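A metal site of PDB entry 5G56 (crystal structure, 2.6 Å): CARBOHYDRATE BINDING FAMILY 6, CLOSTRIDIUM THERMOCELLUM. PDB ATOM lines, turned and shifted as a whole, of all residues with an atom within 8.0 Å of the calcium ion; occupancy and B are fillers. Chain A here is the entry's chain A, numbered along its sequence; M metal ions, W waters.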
ATOM      1  N   ARG A 340      -2.971 -11.144 -18.167  1.00  0.00           N
ATOM      2  CA  ARG A 340      -4.039 -11.724 -18.958  1.00  0.00           C
ATOM      3  C   ARG A 340      -4.238 -10.937 -20.240  1.00  0.00           C
ATOM      4  O   ARG A 340      -4.563  -9.747 -20.193  1.00  0.00           O
ATOM      5  CB  ARG A 340      -5.356 -11.788 -18.184  1.00  0.00           C
ATOM      6  CG  ARG A 340      -6.414 -12.583 -18.933  1.00  0.00           C
ATOM      7  CD  ARG A 340      -7.644 -12.857 -18.102  1.00  0.00           C
ATOM      8  NE  ARG A 340      -7.418 -13.889 -17.098  1.00  0.00           N
ATOM      9  CZ  ARG A 340      -8.384 -14.470 -16.385  1.00  0.00           C
ATOM     10  NH1 ARG A 340      -9.664 -14.137 -16.540  1.00  0.00           N
ATOM     11  NH2 ARG A 340      -8.063 -15.410 -15.503  1.00  0.00           N
ATOM     12  N   ILE A 341      -4.048 -11.612 -21.375  1.00  0.00           N
ATOM     13  CA  ILE A 341      -4.347 -11.065 -22.693  1.00  0.00           C
ATOM     14  C   ILE A 341      -5.643 -11.712 -23.182  1.00  0.00           C
ATOM     15  O   ILE A 341      -5.672 -12.920 -23.492  1.00  0.00           O
ATOM     16  CB  ILE A 341      -3.202 -11.349 -23.697  1.00  0.00           C
ATOM     17  CG1 ILE A 341      -1.849 -10.943 -23.112  1.00  0.00           C
ATOM     18  CG2 ILE A 341      -3.460 -10.640 -25.026  1.00  0.00           C
ATOM     19  CD1 ILE A 341      -0.650 -11.536 -23.837  1.00  0.00           C
ATOM     20  N   GLU A 342      -6.721 -10.928 -23.235  1.00  0.00           N
ATOM     21  CA  GLU A 342      -8.004 -11.426 -23.737  1.00  0.00           C
ATOM     22  C   GLU A 342      -7.866 -11.699 -25.228  1.00  0.00           C
ATOM     23  O   GLU A 342      -7.276 -10.883 -25.949  1.00  0.00           O
ATOM     24  CB  GLU A 342      -9.123 -10.406 -23.511  1.00  0.00           C
ATOM     25  CG  GLU A 342      -9.390 -10.046 -22.048  1.00  0.00           C
ATOM     26  CD  GLU A 342      -9.955 -11.191 -21.233  1.00  0.00           C
ATOM     27  OE1 GLU A 342     -10.524 -12.140 -21.830  1.00  0.00           O
ATOM     28  OE2 GLU A 342      -9.841 -11.141 -19.988  1.00  0.00           O
ATOM     29  N   ALA A 343      -8.389 -12.837 -25.688  1.00  0.00           N
ATOM     30  CA  ALA A 343      -8.226 -13.287 -27.079  1.00  0.00           C
ATOM     31  C   ALA A 343      -8.873 -12.336 -28.096  1.00  0.00           C
ATOM     32  O   ALA A 343      -8.360 -12.164 -29.200  1.00  0.00           O
ATOM     33  CB  ALA A 343      -8.786 -14.690 -27.242  1.00  0.00           C
ATOM     34  N   GLU A 344     -10.005 -11.767 -27.713  1.00  0.00           N
ATOM     35  CA  GLU A 344     -10.720 -10.747 -28.514  1.00  0.00           C
ATOM     36  C   GLU A 344     -10.018  -9.376 -28.613  1.00  0.00           C
ATOM     37  O   GLU A 344     -10.513  -8.508 -29.333  1.00  0.00           O
ATOM     38  CB  GLU A 344     -12.170 -10.565 -27.994  1.00  0.00           C
ATOM     39  CG  GLU A 344     -12.328  -9.934 -26.605  1.00  0.00           C
ATOM     40  CD  GLU A 344     -12.360 -10.942 -25.449  1.00  0.00           C
ATOM     41  OE1 GLU A 344     -11.783 -12.045 -25.540  1.00  0.00           O
ATOM     42  OE2 GLU A 344     -12.952 -10.633 -24.396  1.00  0.00           O
ATOM     43  N   ASP A 345      -8.901  -9.183 -27.896  1.00  0.00           N
ATOM     44  CA  ASP A 345      -8.051  -7.975 -28.023  1.00  0.00           C
ATOM     45  C   ASP A 345      -6.812  -8.180 -28.924  1.00  0.00           C
ATOM     46  O   ASP A 345      -5.798  -7.521 -28.737  1.00  0.00           O
ATOM     47  CB  ASP A 345      -7.590  -7.492 -26.637  1.00  0.00           C
ATOM     48  CG  ASP A 345      -8.744  -7.059 -25.752  1.00  0.00           C
ATOM     49  OD1 ASP A 345      -9.812  -6.728 -26.275  1.00  0.00           O
ATOM     50  OD2 ASP A 345      -8.547  -7.058 -24.515  1.00  0.00           O
ATOM     51  N   TYR A 367     -18.460  -7.040 -29.805  1.00  0.00           N
ATOM     52  CA  TYR A 367     -17.169  -6.409 -29.480  1.00  0.00           C
ATOM     53  C   TYR A 367     -16.551  -5.572 -30.588  1.00  0.00           C
ATOM     54  O   TYR A 367     -16.267  -4.392 -30.383  1.00  0.00           O
ATOM     55  CB  TYR A 367     -16.160  -7.464 -28.982  1.00  0.00           C
ATOM     56  CG  TYR A 367     -15.056  -6.943 -28.080  1.00  0.00           C
ATOM     57  CD1 TYR A 367     -15.349  -6.345 -26.853  1.00  0.00           C
ATOM     58  CD2 TYR A 367     -13.710  -7.073 -28.430  1.00  0.00           C
ATOM     59  CE1 TYR A 367     -14.346  -5.875 -26.015  1.00  0.00           C
ATOM     60  CE2 TYR A 367     -12.698  -6.606 -27.595  1.00  0.00           C
ATOM     61  CZ  TYR A 367     -13.023  -6.008 -26.390  1.00  0.00           C
ATOM     62  OH  TYR A 367     -12.038  -5.554 -25.557  1.00  0.00           O
ATOM     63  N   ILE A 375     -16.464 -13.219 -32.820  1.00  0.00           N
ATOM     64  CA  ILE A 375     -16.499 -12.950 -31.379  1.00  0.00           C
ATOM     65  C   ILE A 375     -17.935 -13.075 -30.841  1.00  0.00           C
ATOM     66  O   ILE A 375     -18.861 -12.512 -31.406  1.00  0.00           O
ATOM     67  CB  ILE A 375     -15.946 -11.533 -31.111  1.00  0.00           C
ATOM     68  CG1 ILE A 375     -14.659 -11.288 -31.891  1.00  0.00           C
ATOM     69  CG2 ILE A 375     -15.693 -11.317 -29.617  1.00  0.00           C
ATOM     70  CD1 ILE A 375     -14.061  -9.928 -31.683  1.00  0.00           C
ATOM     71  N   GLU A 376     -18.092 -13.833 -29.757  1.00  0.00           N
ATOM     72  CA  GLU A 376     -19.383 -13.977 -29.042  1.00  0.00           C
ATOM     73  C   GLU A 376     -19.191 -13.666 -27.557  1.00  0.00           C
ATOM     74  O   GLU A 376     -18.067 -13.592 -27.080  1.00  0.00           O
ATOM     75  CB  GLU A 376     -19.962 -15.395 -29.210  1.00  0.00           C
ATOM     76  CG  GLU A 376     -19.132 -16.524 -28.588  1.00  0.00           C
ATOM     77  CD  GLU A 376     -19.710 -17.923 -28.798  1.00  0.00           C
ATOM     78  OE1 GLU A 376     -20.945 -18.054 -29.001  1.00  0.00           O
ATOM     79  OE2 GLU A 376     -18.929 -18.902 -28.749  1.00  0.00           O
ATOM     80  N   THR A 378     -19.140 -14.742 -23.706  1.00  0.00           N
ATOM     81  CA  THR A 378     -18.806 -16.002 -23.016  1.00  0.00           C
ATOM     82  C   THR A 378     -19.489 -16.084 -21.658  1.00  0.00           C
ATOM     83  O   THR A 378     -19.771 -15.065 -21.034  1.00  0.00           O
ATOM     84  CB  THR A 378     -17.291 -16.202 -22.843  1.00  0.00           C
ATOM     85  OG1 THR A 378     -17.035 -17.499 -22.283  1.00  0.00           O
ATOM     86  CG2 THR A 378     -16.637 -15.121 -21.966  1.00  0.00           C
ATOM     87  N   ASP A 380     -17.987 -17.795 -19.146  1.00  0.00           N
ATOM     88  CA  ASP A 380     -16.877 -18.263 -18.327  1.00  0.00           C
ATOM     89  C   ASP A 380     -16.631 -17.254 -17.219  1.00  0.00           C
ATOM     90  O   ASP A 380     -16.952 -16.079 -17.369  1.00  0.00           O
ATOM     91  CB  ASP A 380     -15.607 -18.393 -19.188  1.00  0.00           C
ATOM     92  CG  ASP A 380     -14.507 -19.186 -18.501  1.00  0.00           C
ATOM     93  OD1 ASP A 380     -14.806 -20.083 -17.696  1.00  0.00           O
ATOM     94  OD2 ASP A 380     -13.317 -18.910 -18.775  1.00  0.00           O
ATOM     95  N   THR A 381     -16.032 -17.727 -16.119  1.00  0.00           N
ATOM     96  CA  THR A 381     -15.616 -16.864 -14.997  1.00  0.00           C
ATOM     97  C   THR A 381     -14.849 -15.621 -15.463  1.00  0.00           C
ATOM     98  O   THR A 381     -13.886 -15.721 -16.239  1.00  0.00           O
ATOM     99  CB  THR A 381     -14.731 -17.653 -14.009  1.00  0.00           C
ATOM    100  OG1 THR A 381     -15.392 -18.860 -13.623  1.00  0.00           O
ATOM    101  CG2 THR A 381     -14.405 -16.807 -12.763  1.00  0.00           C
ATOM    102  N   GLY A 382     -15.292 -14.448 -14.999  1.00  0.00           N
ATOM    103  CA  GLY A 382     -14.787 -13.160 -15.474  1.00  0.00           C
ATOM    104  C   GLY A 382     -15.583 -12.548 -16.620  1.00  0.00           C
ATOM    105  O   GLY A 382     -15.263 -11.435 -17.064  1.00  0.00           O
ATOM    106  N   GLY A 383     -16.596 -13.255 -17.117  1.00  0.00           N
ATOM    107  CA  GLY A 383     -17.480 -12.759 -18.157  1.00  0.00           C
ATOM    108  C   GLY A 383     -16.739 -12.359 -19.423  1.00  0.00           C
ATOM    109  O   GLY A 383     -15.774 -13.028 -19.823  1.00  0.00           O
ATOM    110  N   GLY A 384     -17.200 -11.286 -20.042  1.00  0.00           N
ATOM    111  CA  GLY A 384     -16.636 -10.772 -21.283  1.00  0.00           C
ATOM    112  C   GLY A 384     -16.972 -11.627 -22.490  1.00  0.00           C
ATOM    113  O   GLY A 384     -18.050 -12.221 -22.555  1.00  0.00           O
ATOM    114  N   TYR A 385     -16.021 -11.703 -23.425  1.00  0.00           N
ATOM    115  CA  TYR A 385     -16.233 -12.294 -24.751  1.00  0.00           C
ATOM    116  C   TYR A 385     -15.223 -13.411 -25.019  1.00  0.00           C
ATOM    117  O   TYR A 385     -14.188 -13.476 -24.365  1.00  0.00           O
ATOM    118  CB  TYR A 385     -16.129 -11.209 -25.828  1.00  0.00           C
ATOM    119  CG  TYR A 385     -17.000 -10.004 -25.545  1.00  0.00           C
ATOM    120  CD1 TYR A 385     -18.323  -9.958 -25.973  1.00  0.00           C
ATOM    121  CD2 TYR A 385     -16.508  -8.917 -24.812  1.00  0.00           C
ATOM    122  CE1 TYR A 385     -19.133  -8.861 -25.699  1.00  0.00           C
ATOM    123  CE2 TYR A 385     -17.313  -7.816 -24.531  1.00  0.00           C
ATOM    124  CZ  TYR A 385     -18.629  -7.794 -24.975  1.00  0.00           C
ATOM    125  OH  TYR A 385     -19.412  -6.693 -24.694  1.00  0.00           O
ATOM    126  N   ASN A 386     -15.560 -14.296 -25.959  1.00  0.00           N
ATOM    127  CA  ASN A 386     -14.614 -15.295 -26.482  1.00  0.00           C
ATOM    128  C   ASN A 386     -14.557 -15.263 -28.015  1.00  0.00           C
ATOM    129  O   ASN A 386     -15.574 -15.035 -28.681  1.00  0.00           O
ATOM    130  CB  ASN A 386     -14.934 -16.703 -25.952  1.00  0.00           C
ATOM    131  CG  ASN A 386     -16.166 -17.329 -26.579  1.00  0.00           C
ATOM    132  OD1 ASN A 386     -17.269 -17.267 -26.026  1.00  0.00           O
ATOM    133  ND2 ASN A 386     -15.992 -17.973 -27.724  1.00  0.00           N
ATOM    134  N   VAL A 387     -13.360 -15.486 -28.562  1.00  0.00           N
ATOM    135  CA  VAL A 387     -13.195 -15.747 -29.998  1.00  0.00           C
ATOM    136  C   VAL A 387     -13.733 -17.146 -30.275  1.00  0.00           C
ATOM    137  O   VAL A 387     -13.297 -18.110 -29.643  1.00  0.00           O
ATOM    138  CB  VAL A 387     -11.708 -15.675 -30.452  1.00  0.00           C
ATOM    139  CG1 VAL A 387     -11.541 -16.142 -31.902  1.00  0.00           C
ATOM    140  CG2 VAL A 387     -11.177 -14.251 -30.297  1.00  0.00           C
ATOM    141  N   ARG A 413      -6.896 -20.409 -22.111  1.00  0.00           N
ATOM    142  CA  ARG A 413      -8.216 -20.762 -21.592  1.00  0.00           C
ATOM    143  C   ARG A 413      -9.082 -21.185 -22.770  1.00  0.00           C
ATOM    144  O   ARG A 413      -9.423 -20.361 -23.628  1.00  0.00           O
ATOM    145  CB  ARG A 413      -8.832 -19.553 -20.864  1.00  0.00           C
ATOM    146  CG  ARG A 413     -10.142 -19.805 -20.132  1.00  0.00           C
ATOM    147  CD  ARG A 413      -9.936 -20.708 -18.927  1.00  0.00           C
ATOM    148  NE  ARG A 413     -11.134 -20.892 -18.122  1.00  0.00           N
ATOM    149  CZ  ARG A 413     -11.226 -21.696 -17.063  1.00  0.00           C
ATOM    150  NH1 ARG A 413     -10.185 -22.424 -16.654  1.00  0.00           N
ATOM    151  NH2 ARG A 413     -12.375 -21.790 -16.405  1.00  0.00           N
ATOM    152  N   TRP A 446     -15.117 -24.631 -20.080  1.00  0.00           N
ATOM    153  CA  TRP A 446     -13.772 -24.075 -20.135  1.00  0.00           C
ATOM    154  C   TRP A 446     -12.759 -24.826 -19.256  1.00  0.00           C
ATOM    155  O   TRP A 446     -13.090 -25.343 -18.192  1.00  0.00           O
ATOM    156  CB  TRP A 446     -13.811 -22.583 -19.792  1.00  0.00           C
ATOM    157  CG  TRP A 446     -14.602 -21.791 -20.802  1.00  0.00           C
ATOM    158  CD1 TRP A 446     -15.918 -21.470 -20.735  1.00  0.00           C
ATOM    159  CD2 TRP A 446     -14.122 -21.258 -22.042  1.00  0.00           C
ATOM    160  NE1 TRP A 446     -16.302 -20.760 -21.845  1.00  0.00           N
ATOM    161  CE2 TRP A 446     -15.213 -20.615 -22.662  1.00  0.00           C
ATOM    162  CE3 TRP A 446     -12.871 -21.254 -22.679  1.00  0.00           C
ATOM    163  CZ2 TRP A 446     -15.094 -19.976 -23.902  1.00  0.00           C
ATOM    164  CZ3 TRP A 446     -12.753 -20.623 -23.913  1.00  0.00           C
ATOM    165  CH2 TRP A 446     -13.863 -19.990 -24.515  1.00  0.00           C
ATOM    166  N   LEU A 473     -11.699 -19.730 -27.828  1.00  0.00           N
ATOM    167  CA  LEU A 473     -10.608 -19.143 -27.042  1.00  0.00           C
ATOM    168  C   LEU A 473     -11.064 -17.876 -26.306  1.00  0.00           C
ATOM    169  O   LEU A 473     -11.486 -16.902 -26.939  1.00  0.00           O
ATOM    170  CB  LEU A 473      -9.428 -18.816 -27.958  1.00  0.00           C
ATOM    171  CG  LEU A 473      -8.120 -18.345 -27.318  1.00  0.00           C
ATOM    172  CD1 LEU A 473      -7.455 -19.458 -26.531  1.00  0.00           C
ATOM    173  CD2 LEU A 473      -7.170 -17.816 -28.383  1.00  0.00           C
ATOM    174  N   ASN A 474     -10.954 -17.896 -24.985  1.00  0.00           N
ATOM    175  CA  ASN A 474     -11.375 -16.790 -24.109  1.00  0.00           C
ATOM    176  C   ASN A 474     -10.217 -15.820 -23.868  1.00  0.00           C
ATOM    177  O   ASN A 474     -10.345 -14.632 -24.139  1.00  0.00           O
ATOM    178  CB  ASN A 474     -11.889 -17.366 -22.778  1.00  0.00           C
ATOM    179  CG  ASN A 474     -12.486 -16.294 -21.861  1.00  0.00           C
ATOM    180  OD1 ASN A 474     -12.466 -15.108 -22.157  1.00  0.00           O
ATOM    181  ND2 ASN A 474     -13.014 -16.740 -20.729  1.00  0.00           N
ATOM    182  N   TRP A 475      -9.108 -16.323 -23.325  1.00  0.00           N
ATOM    183  CA  TRP A 475      -7.941 -15.494 -23.024  1.00  0.00           C
ATOM    184  C   TRP A 475      -6.624 -16.269 -23.008  1.00  0.00           C
ATOM    185  O   TRP A 475      -6.602 -17.505 -23.005  1.00  0.00           O
ATOM    186  CB  TRP A 475      -8.108 -14.729 -21.690  1.00  0.00           C
ATOM    187  CG  TRP A 475      -8.545 -15.533 -20.502  1.00  0.00           C
ATOM    188  CD1 TRP A 475      -9.782 -15.525 -19.950  1.00  0.00           C
ATOM    189  CD2 TRP A 475      -7.746 -16.419 -19.694  1.00  0.00           C
ATOM    190  NE1 TRP A 475      -9.827 -16.367 -18.855  1.00  0.00           N
ATOM    191  CE2 TRP A 475      -8.592 -16.924 -18.673  1.00  0.00           C
ATOM    192  CE3 TRP A 475      -6.409 -16.843 -19.734  1.00  0.00           C
ATOM    193  CZ2 TRP A 475      -8.135 -17.829 -17.712  1.00  0.00           C
ATOM    194  CZ3 TRP A 475      -5.957 -17.762 -18.774  1.00  0.00           C
ATOM    195  CH2 TRP A 475      -6.823 -18.241 -17.770  1.00  0.00           C
ATOM    196  N   ILE A 476      -5.540 -15.499 -23.023  1.00  0.00           N
ATOM    197  CA  ILE A 476      -4.180 -15.997 -22.973  1.00  0.00           C
ATOM    198  C   ILE A 476      -3.520 -15.418 -21.712  1.00  0.00           C
ATOM    199  O   ILE A 476      -3.846 -14.310 -21.295  1.00  0.00           O
ATOM    200  CB  ILE A 476      -3.414 -15.553 -24.244  1.00  0.00           C
ATOM    201  CG1 ILE A 476      -4.131 -16.033 -25.508  1.00  0.00           C
ATOM    202  CG2 ILE A 476      -1.980 -16.084 -24.235  1.00  0.00           C
ATOM    203  CD1 ILE A 476      -3.903 -15.144 -26.697  1.00  0.00           C
HETATM  204 CA    CA M   1     -12.107 -13.031 -23.350  1.00  0.00          CA
HETATM  205  O   HOH W   1     -13.535 -12.069 -21.737  1.00  0.00           O
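ND2 of Asn 474 lies within hydrogen-bond range of OD2 of Asp 380.
The backbone NH (N) of Asn 474 is in hydrogen-bond range of the backbone carbonyl oxygen (O) of Arg 413, at 3.2 Å.
The backbone carbonyl oxygen (O) of Asn 474 lies close to the backbone NH (N) of Ala 343 (3.1 Å).
The calcium ion is bound by O of Tyr 385, at 2.4 Å.
The calcium ion is bound by water W1, 2.4 Å away.
The side-chain carboxylate (OE1) of Glu 342 binds the calcium ion, 2.4 Å away.
The calcium ion is bound by the side-chain amide oxygen (OD1) of Asn 474 (2.4 Å).
The calcium ion is bound by OE1 of Glu 344 (2.4 Å).
The calcium ion is bound by O of Asn 474 (2.5 Å).
The calcium ion is bound by the side-chain carboxylate (OE2) of Glu 344 (2.7 Å).
The calcium ion has seven donor atoms within binding distance.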
